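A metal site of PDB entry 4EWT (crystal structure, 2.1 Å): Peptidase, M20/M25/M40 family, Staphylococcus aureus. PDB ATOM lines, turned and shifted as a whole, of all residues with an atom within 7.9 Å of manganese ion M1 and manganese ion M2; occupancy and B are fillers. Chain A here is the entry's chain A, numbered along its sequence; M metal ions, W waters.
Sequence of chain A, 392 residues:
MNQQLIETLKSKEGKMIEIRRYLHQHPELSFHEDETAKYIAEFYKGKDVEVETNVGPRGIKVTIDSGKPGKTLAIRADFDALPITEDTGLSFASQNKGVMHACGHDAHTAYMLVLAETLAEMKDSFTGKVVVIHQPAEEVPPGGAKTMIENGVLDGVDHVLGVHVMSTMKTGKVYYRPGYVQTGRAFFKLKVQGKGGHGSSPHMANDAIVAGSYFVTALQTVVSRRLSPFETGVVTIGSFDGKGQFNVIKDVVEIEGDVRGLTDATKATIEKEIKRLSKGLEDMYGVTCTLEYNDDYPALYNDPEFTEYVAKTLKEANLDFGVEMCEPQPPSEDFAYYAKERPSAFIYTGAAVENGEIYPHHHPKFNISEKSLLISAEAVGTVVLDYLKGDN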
ATOM      1  N   ARG A  76      22.809 -14.292  13.981  1.00  0.00           N
ATOM      2  CA  ARG A  76      21.751 -14.017  14.944  1.00  0.00           C
ATOM      3  C   ARG A  76      21.944 -12.699  15.697  1.00  0.00           C
ATOM      4  O   ARG A  76      23.042 -12.405  16.169  1.00  0.00           O
ATOM      5  CB  ARG A  76      21.617 -15.202  15.908  1.00  0.00           C
ATOM      6  CG  ARG A  76      20.543 -15.079  16.955  1.00  0.00           C
ATOM      7  CD  ARG A  76      21.038 -14.363  18.203  1.00  0.00           C
ATOM      8  NE  ARG A  76      20.229 -14.767  19.343  1.00  0.00           N
ATOM      9  CZ  ARG A  76      20.594 -14.646  20.619  1.00  0.00           C
ATOM     10  NH1 ARG A  76      21.779 -14.115  20.960  1.00  0.00           N
ATOM     11  NH2 ARG A  76      19.771 -15.080  21.559  1.00  0.00           N
ATOM     12  N   ASP A  78      19.590 -10.444  18.684  1.00  0.00           N
ATOM     13  CA  ASP A  78      18.384 -10.314  19.518  1.00  0.00           C
ATOM     14  C   ASP A  78      17.983  -8.845  19.677  1.00  0.00           C
ATOM     15  O   ASP A  78      18.810  -7.939  19.494  1.00  0.00           O
ATOM     16  CB  ASP A  78      18.530 -11.028  20.880  1.00  0.00           C
ATOM     17  CG  ASP A  78      19.914 -10.864  21.500  1.00  0.00           C
ATOM     18  OD1 ASP A  78      20.762 -10.102  20.979  1.00  0.00           O
ATOM     19  OD2 ASP A  78      20.165 -11.500  22.537  1.00  0.00           O
ATOM     20  N   ASP A  80      15.092  -7.718  22.174  1.00  0.00           N
ATOM     21  CA  ASP A  80      14.294  -7.387  23.360  1.00  0.00           C
ATOM     22  C   ASP A  80      15.105  -6.572  24.374  1.00  0.00           C
ATOM     23  O   ASP A  80      16.337  -6.693  24.434  1.00  0.00           O
ATOM     24  CB  ASP A  80      13.697  -8.636  24.033  1.00  0.00           C
ATOM     25  CG  ASP A  80      14.769  -9.646  24.478  1.00  0.00           C
ATOM     26  OD1 ASP A  80      15.837  -9.756  23.831  1.00  0.00           O
ATOM     27  OD2 ASP A  80      14.515 -10.352  25.479  1.00  0.00           O
ATOM     28  N   ALA A  81      14.405  -5.746  25.133  1.00  0.00           N
ATOM     29  CA  ALA A  81      15.021  -4.929  26.189  1.00  0.00           C
ATOM     30  C   ALA A  81      14.653  -5.470  27.579  1.00  0.00           C
ATOM     31  O   ALA A  81      14.047  -6.533  27.681  1.00  0.00           O
ATOM     32  CB  ALA A  81      14.607  -3.487  26.040  1.00  0.00           C
ATOM     33  N   LEU A  82      15.007  -4.729  28.626  1.00  0.00           N
ATOM     34  CA  LEU A  82      14.838  -5.181  30.019  1.00  0.00           C
ATOM     35  C   LEU A  82      14.006  -4.212  30.873  1.00  0.00           C
ATOM     36  O   LEU A  82      13.931  -3.022  30.561  1.00  0.00           O
ATOM     37  CB  LEU A  82      16.210  -5.382  30.663  1.00  0.00           C
ATOM     38  CG  LEU A  82      17.059  -6.562  30.205  1.00  0.00           C
ATOM     39  CD1 LEU A  82      18.531  -6.236  30.370  1.00  0.00           C
ATOM     40  CD2 LEU A  82      16.685  -7.815  30.978  1.00  0.00           C
ATOM     41  N   ILE A  84      14.225  -2.059  33.284  1.00  0.00           N
ATOM     42  CA  ILE A  84      15.230  -1.286  34.008  1.00  0.00           C
ATOM     43  C   ILE A  84      15.079   0.212  33.702  1.00  0.00           C
ATOM     44  O   ILE A  84      14.943   0.591  32.533  1.00  0.00           O
ATOM     45  CB  ILE A  84      16.670  -1.763  33.648  1.00  0.00           C
ATOM     46  CG1 ILE A  84      16.935  -3.170  34.217  1.00  0.00           C
ATOM     47  CG2 ILE A  84      17.730  -0.778  34.141  1.00  0.00           C
ATOM     48  CD1 ILE A  84      17.951  -3.964  33.445  1.00  0.00           C
ATOM     49  N   ALA A 102      19.584  -2.523  28.184  1.00  0.00           N
ATOM     50  CA  ALA A 102      20.720  -2.623  29.105  1.00  0.00           C
ATOM     51  C   ALA A 102      21.672  -3.792  28.811  1.00  0.00           C
ATOM     52  O   ALA A 102      22.533  -4.097  29.641  1.00  0.00           O
ATOM     53  CB  ALA A 102      20.206  -2.698  30.565  1.00  0.00           C
ATOM     54  N   CYS A 103      21.517  -4.416  27.643  1.00  0.00           N
ATOM     55  CA  CYS A 103      22.367  -5.566  27.246  1.00  0.00           C
ATOM     56  C   CYS A 103      22.921  -5.439  25.819  1.00  0.00           C
ATOM     57  O   CYS A 103      23.537  -6.373  25.300  1.00  0.00           O
ATOM     58  CB  CYS A 103      21.591  -6.889  27.396  1.00  0.00           C
ATOM     59  SG  CYS A 103      22.626  -8.338  27.778  1.00  0.00           S
ATOM     60  N   GLY A 104      22.707  -4.288  25.193  1.00  0.00           N
ATOM     61  CA  GLY A 104      23.282  -3.981  23.884  1.00  0.00           C
ATOM     62  C   GLY A 104      22.546  -4.631  22.730  1.00  0.00           C
ATOM     63  O   GLY A 104      23.088  -4.707  21.622  1.00  0.00           O
ATOM     64  N   HIS A 105      21.318  -5.084  22.972  1.00  0.00           N
ATOM     65  CA  HIS A 105      20.500  -5.717  21.934  1.00  0.00           C
ATOM     66  C   HIS A 105      20.116  -4.724  20.833  1.00  0.00           C
ATOM     67  O   HIS A 105      19.945  -5.103  19.672  1.00  0.00           O
ATOM     68  CB  HIS A 105      19.234  -6.340  22.547  1.00  0.00           C
ATOM     69  CG  HIS A 105      19.501  -7.525  23.422  1.00  0.00           C
ATOM     70  ND1 HIS A 105      18.486  -8.323  23.893  1.00  0.00           N
ATOM     71  CD2 HIS A 105      20.650  -8.046  23.914  1.00  0.00           C
ATOM     72  CE1 HIS A 105      18.993  -9.290  24.638  1.00  0.00           C
ATOM     73  NE2 HIS A 105      20.310  -9.139  24.668  1.00  0.00           N
ATOM     74  N   HIS A 108      23.201  -4.857  18.768  1.00  0.00           N
ATOM     75  CA  HIS A 108      23.177  -6.077  17.965  1.00  0.00           C
ATOM     76  C   HIS A 108      22.272  -5.933  16.730  1.00  0.00           C
ATOM     77  O   HIS A 108      22.645  -6.324  15.623  1.00  0.00           O
ATOM     78  CB  HIS A 108      22.763  -7.286  18.791  1.00  0.00           C
ATOM     79  CG  HIS A 108      23.633  -7.532  19.982  1.00  0.00           C
ATOM     80  ND1 HIS A 108      23.203  -8.220  21.094  1.00  0.00           N
ATOM     81  CD2 HIS A 108      24.920  -7.182  20.242  1.00  0.00           C
ATOM     82  CE1 HIS A 108      24.180  -8.280  21.988  1.00  0.00           C
ATOM     83  NE2 HIS A 108      25.230  -7.654  21.491  1.00  0.00           N
ATOM     84  N   GLU A 138      14.803 -12.827  24.273  1.00  0.00           N
ATOM     85  CA  GLU A 138      16.015 -13.503  24.753  1.00  0.00           C
ATOM     86  C   GLU A 138      16.105 -13.502  26.291  1.00  0.00           C
ATOM     87  O   GLU A 138      16.558 -14.474  26.882  1.00  0.00           O
ATOM     88  CB  GLU A 138      17.271 -12.855  24.130  1.00  0.00           C
ATOM     89  CG  GLU A 138      18.603 -13.574  24.425  1.00  0.00           C
ATOM     90  CD  GLU A 138      19.173 -13.300  25.811  1.00  0.00           C
ATOM     91  OE1 GLU A 138      18.994 -12.175  26.330  1.00  0.00           O
ATOM     92  OE2 GLU A 138      19.804 -14.220  26.391  1.00  0.00           O
ATOM     93  N   GLU A 139      15.657 -12.423  26.913  1.00  0.00           N
ATOM     94  CA  GLU A 139      15.941 -12.142  28.324  1.00  0.00           C
ATOM     95  C   GLU A 139      15.108 -12.901  29.352  1.00  0.00           C
ATOM     96  O   GLU A 139      15.555 -13.110  30.488  1.00  0.00           O
ATOM     97  CB  GLU A 139      15.843 -10.639  28.600  1.00  0.00           C
ATOM     98  CG  GLU A 139      16.889  -9.819  27.862  1.00  0.00           C
ATOM     99  CD  GLU A 139      18.298  -9.981  28.438  1.00  0.00           C
ATOM    100  OE1 GLU A 139      18.524 -10.859  29.298  1.00  0.00           O
ATOM    101  OE2 GLU A 139      19.185  -9.207  28.021  1.00  0.00           O
ATOM    102  N   VAL A 163      26.918 -12.818  17.887  1.00  0.00           N
ATOM    103  CA  VAL A 163      27.867 -11.911  18.489  1.00  0.00           C
ATOM    104  C   VAL A 163      27.150 -11.210  19.613  1.00  0.00           C
ATOM    105  O   VAL A 163      25.974 -10.885  19.502  1.00  0.00           O
ATOM    106  CB  VAL A 163      28.411 -10.876  17.458  1.00  0.00           C
ATOM    107  CG1 VAL A 163      29.018  -9.664  18.172  1.00  0.00           C
ATOM    108  CG2 VAL A 163      29.432 -11.512  16.560  1.00  0.00           C
ATOM    109  N   HIS A 164      27.871 -11.006  20.724  1.00  0.00           N
ATOM    110  CA  HIS A 164      27.395 -10.162  21.798  1.00  0.00           C
ATOM    111  C   HIS A 164      28.460  -9.114  22.081  1.00  0.00           C
ATOM    112  O   HIS A 164      29.647  -9.445  22.232  1.00  0.00           O
ATOM    113  CB  HIS A 164      27.125 -10.991  23.054  1.00  0.00           C
ATOM    114  CG  HIS A 164      26.038 -10.441  23.921  1.00  0.00           C
ATOM    115  ND1 HIS A 164      26.187  -9.287  24.650  1.00  0.00           N
ATOM    116  CD2 HIS A 164      24.787 -10.885  24.167  1.00  0.00           C
ATOM    117  CE1 HIS A 164      25.080  -9.047  25.321  1.00  0.00           C
ATOM    118  NE2 HIS A 164      24.210 -10.011  25.055  1.00  0.00           N
ATOM    119  N   VAL A 165      28.034  -7.848  22.126  1.00  0.00           N
ATOM    120  CA  VAL A 165      28.877  -6.766  22.638  1.00  0.00           C
ATOM    121  C   VAL A 165      29.102  -6.951  24.136  1.00  0.00           C
ATOM    122  O   VAL A 165      28.185  -7.308  24.879  1.00  0.00           O
ATOM    123  CB  VAL A 165      28.260  -5.372  22.382  1.00  0.00           C
ATOM    124  CG1 VAL A 165      28.246  -5.035  20.893  1.00  0.00           C
ATOM    125  CG2 VAL A 165      26.834  -5.264  22.994  1.00  0.00           C
ATOM    126  N   MET A 166      30.343  -6.735  24.566  1.00  0.00           N
ATOM    127  CA  MET A 166      30.711  -6.867  25.963  1.00  0.00           C
ATOM    128  C   MET A 166      31.226  -5.557  26.536  1.00  0.00           C
ATOM    129  O   MET A 166      32.356  -5.148  26.262  1.00  0.00           O
ATOM    130  CB  MET A 166      31.747  -7.973  26.134  1.00  0.00           C
ATOM    131  CG  MET A 166      31.284  -9.335  25.643  1.00  0.00           C
ATOM    132  SD  MET A 166      29.833  -9.962  26.499  1.00  0.00           S
ATOM    133  CE  MET A 166      30.593 -10.853  27.847  1.00  0.00           C
ATOM    134  N   GLN A 182      29.158 -20.128  28.192  1.00  0.00           N
ATOM    135  CA  GLN A 182      28.212 -19.468  29.116  1.00  0.00           C
ATOM    136  C   GLN A 182      27.365 -20.504  29.836  1.00  0.00           C
ATOM    137  O   GLN A 182      27.071 -21.553  29.295  1.00  0.00           O
ATOM    138  CB  GLN A 182      27.363 -18.416  28.385  1.00  0.00           C
ATOM    139  CG  GLN A 182      28.207 -17.204  28.029  1.00  0.00           C
ATOM    140  CD  GLN A 182      27.467 -16.009  27.486  1.00  0.00           C
ATOM    141  OE1 GLN A 182      27.926 -15.395  26.536  1.00  0.00           O
ATOM    142  NE2 GLN A 182      26.351 -15.640  28.103  1.00  0.00           N
ATOM    143  N   PRO A 331      26.868 -14.938  32.650  1.00  0.00           N
ATOM    144  CA  PRO A 331      25.415 -14.954  32.410  1.00  0.00           C
ATOM    145  C   PRO A 331      24.934 -16.096  31.502  1.00  0.00           C
ATOM    146  O   PRO A 331      25.721 -16.676  30.751  1.00  0.00           O
ATOM    147  CB  PRO A 331      25.154 -13.599  31.757  1.00  0.00           C
ATOM    148  CG  PRO A 331      26.405 -13.233  31.113  1.00  0.00           C
ATOM    149  CD  PRO A 331      27.512 -13.826  31.944  1.00  0.00           C
ATOM    150  N   SER A 332      23.647 -16.416  31.572  1.00  0.00           N
ATOM    151  CA  SER A 332      23.082 -17.404  30.676  1.00  0.00           C
ATOM    152  C   SER A 332      22.585 -16.653  29.450  1.00  0.00           C
ATOM    153  O   SER A 332      22.379 -15.432  29.483  1.00  0.00           O
ATOM    154  CB  SER A 332      21.971 -18.222  31.355  1.00  0.00           C
ATOM    155  OG  SER A 332      20.701 -17.678  31.041  1.00  0.00           O
ATOM    156  N   GLU A 333      22.408 -17.381  28.352  1.00  0.00           N
ATOM    157  CA  GLU A 333      22.142 -16.785  27.064  1.00  0.00           C
ATOM    158  C   GLU A 333      21.316 -17.798  26.275  1.00  0.00           C
ATOM    159  O   GLU A 333      21.693 -18.976  26.194  1.00  0.00           O
ATOM    160  CB  GLU A 333      23.492 -16.499  26.380  1.00  0.00           C
ATOM    161  CG  GLU A 333      23.457 -16.218  24.894  1.00  0.00           C
ATOM    162  CD  GLU A 333      22.646 -15.011  24.532  1.00  0.00           C
ATOM    163  OE1 GLU A 333      22.938 -13.916  25.068  1.00  0.00           O
ATOM    164  OE2 GLU A 333      21.712 -15.149  23.706  1.00  0.00           O
ATOM    165  N   ASP A 334      20.189 -17.362  25.700  1.00  0.00           N
ATOM    166  CA  ASP A 334      19.346 -18.322  24.991  1.00  0.00           C
ATOM    167  C   ASP A 334      19.817 -18.709  23.584  1.00  0.00           C
ATOM    168  O   ASP A 334      19.267 -19.628  22.975  1.00  0.00           O
ATOM    169  CB  ASP A 334      17.845 -17.992  25.098  1.00  0.00           C
ATOM    170  CG  ASP A 334      17.303 -17.233  23.901  1.00  0.00           C
ATOM    171  OD1 ASP A 334      18.082 -16.657  23.115  1.00  0.00           O
ATOM    172  OD2 ASP A 334      16.054 -17.201  23.767  1.00  0.00           O
ATOM    173  N   PHE A 346      29.298 -18.503  19.415  1.00  0.00           N
ATOM    174  CA  PHE A 346      28.838 -17.232  19.960  1.00  0.00           C
ATOM    175  C   PHE A 346      30.094 -16.503  20.348  1.00  0.00           C
ATOM    176  O   PHE A 346      30.854 -16.989  21.192  1.00  0.00           O
ATOM    177  CB  PHE A 346      27.941 -17.494  21.169  1.00  0.00           C
ATOM    178  CG  PHE A 346      27.168 -16.290  21.653  1.00  0.00           C
ATOM    179  CD1 PHE A 346      26.187 -15.694  20.847  1.00  0.00           C
ATOM    180  CD2 PHE A 346      27.396 -15.778  22.917  1.00  0.00           C
ATOM    181  CE1 PHE A 346      25.452 -14.592  21.317  1.00  0.00           C
ATOM    182  CE2 PHE A 346      26.658 -14.681  23.399  1.00  0.00           C
ATOM    183  CZ  PHE A 346      25.690 -14.087  22.597  1.00  0.00           C
ATOM    184  N   HIS A 361      26.494  -5.365  32.287  1.00  0.00           N
ATOM    185  CA  HIS A 361      25.165  -5.543  31.678  1.00  0.00           C
ATOM    186  C   HIS A 361      24.033  -5.583  32.697  1.00  0.00           C
ATOM    187  O   HIS A 361      24.228  -6.026  33.842  1.00  0.00           O
ATOM    188  CB  HIS A 361      25.142  -6.810  30.832  1.00  0.00           C
ATOM    189  CG  HIS A 361      25.998  -6.724  29.602  1.00  0.00           C
ATOM    190  ND1 HIS A 361      27.369  -6.568  29.651  1.00  0.00           N
ATOM    191  CD2 HIS A 361      25.679  -6.785  28.285  1.00  0.00           C
ATOM    192  CE1 HIS A 361      27.846  -6.521  28.421  1.00  0.00           C
ATOM    193  NE2 HIS A 361      26.845  -6.644  27.580  1.00  0.00           N
ATOM    194  N   HIS A 362      22.861  -5.111  32.273  1.00  0.00           N
ATOM    195  CA  HIS A 362      21.656  -4.998  33.124  1.00  0.00           C
ATOM    196  C   HIS A 362      21.680  -3.872  34.161  1.00  0.00           C
ATOM    197  O   HIS A 362      20.676  -3.613  34.816  1.00  0.00           O
ATOM    198  CB  HIS A 362      21.368  -6.320  33.857  1.00  0.00           C
ATOM    199  CG  HIS A 362      20.922  -7.426  32.967  1.00  0.00           C
ATOM    200  ND1 HIS A 362      19.839  -8.228  33.256  1.00  0.00           N
ATOM    201  CD2 HIS A 362      21.419  -7.882  31.787  1.00  0.00           C
ATOM    202  CE1 HIS A 362      19.681  -9.121  32.304  1.00  0.00           C
ATOM    203  NE2 HIS A 362      20.629  -8.933  31.390  1.00  0.00           N
ATOM    204  N   PHE A 366      24.625   1.123  32.302  1.00  0.00           N
ATOM    205  CA  PHE A 366      25.214   0.360  31.192  1.00  0.00           C
ATOM    206  C   PHE A 366      25.452   1.215  29.953  1.00  0.00           C
ATOM    207  O   PHE A 366      24.554   1.911  29.492  1.00  0.00           O
ATOM    208  CB  PHE A 366      24.294  -0.821  30.846  1.00  0.00           C
ATOM    209  CG  PHE A 366      24.702  -1.595  29.620  1.00  0.00           C
ATOM    210  CD1 PHE A 366      25.634  -2.627  29.709  1.00  0.00           C
ATOM    211  CD2 PHE A 366      24.137  -1.311  28.373  1.00  0.00           C
ATOM    212  CE1 PHE A 366      26.012  -3.353  28.580  1.00  0.00           C
ATOM    213  CE2 PHE A 366      24.510  -2.026  27.239  1.00  0.00           C
ATOM    214  CZ  PHE A 366      25.438  -3.053  27.345  1.00  0.00           C
HETATM  215 MN    MN M   1      21.038  -9.690  29.043  1.00  0.00          MN
HETATM  216 MN    MN M   2      22.080  -9.986  25.842  1.00  0.00          MN
HETATM  217  O   HOH W   1      21.037 -11.538  27.468  1.00  0.00           O
HETATM  218  O   HOH W   2      23.964 -10.318  30.503  1.00  0.00           O
HETATM  219  O   HOH W   3      21.761 -11.622  24.316  1.00  0.00           O
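The backbone NH of Glu 139 is in hydrogen-bond range of the side-chain carboxylate of Asp 80, 2.8 Å away.
A ring nitrogen (NE2) of His 105 lies close to the side-chain carboxylate (OD2) of Asp 78, 3.2 Å away.
The backbone carbonyl oxygen (O) of Asp 80 is in hydrogen-bond range of a ring nitrogen (ND1) of His 105, 2.8 Å away.
O of Ala 102 sits at hydrogen-bond distance from N of His 362 (2.8 Å).
N of Glu 138 is in hydrogen-bond range of OD2 of Asp 80.
The backbone NH (N) of Asp 334 is in hydrogen-bond range of the side-chain carboxylate (OE2) of Glu 138 (3.2 Å).
Residues that only touch manganese ion M2: Glu 138.
Five residues have an atom within 4 Å of manganese ion M2: Cys 103, His 105, Glu 138, Glu 139 and His 164.
The nearest printed residue that does not touch manganese ion M2 is Glu 333 (4.1 Å).
Manganese ion M1 is bound by OE2 of Glu 139, water W1, SG of Cys 103 and NE2 of His 362.
Slightly farther from manganese ion M1 lies OE1 of Glu 139 (2.8 Å).
Manganese ion M2 is bound by water W3 (2.3 Å).
Manganese ion M2 is bound by NE2 of His 164 (2.3 Å).
NE2 of His 105 is bound to manganese ion M2, 2.3 Å away.
Manganese ion M2 is bound by water W1, 2.5 Å away.
The side-chain sulfur (SG) of Cys 103 is bound to manganese ion M2, 2.6 Å away.
Manganese ion M2 has five donor atoms within binding distance.
Water W1 lies within hydrogen-bond range of OE1 of Glu 138 and OE1 of Glu 139.
Water W3 lies within hydrogen-bond range of the side-chain carboxylate (OE1) of Glu 333 (2.7 Å) and the side-chain carboxylate (OE1) of Glu 138 (3.5 Å).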
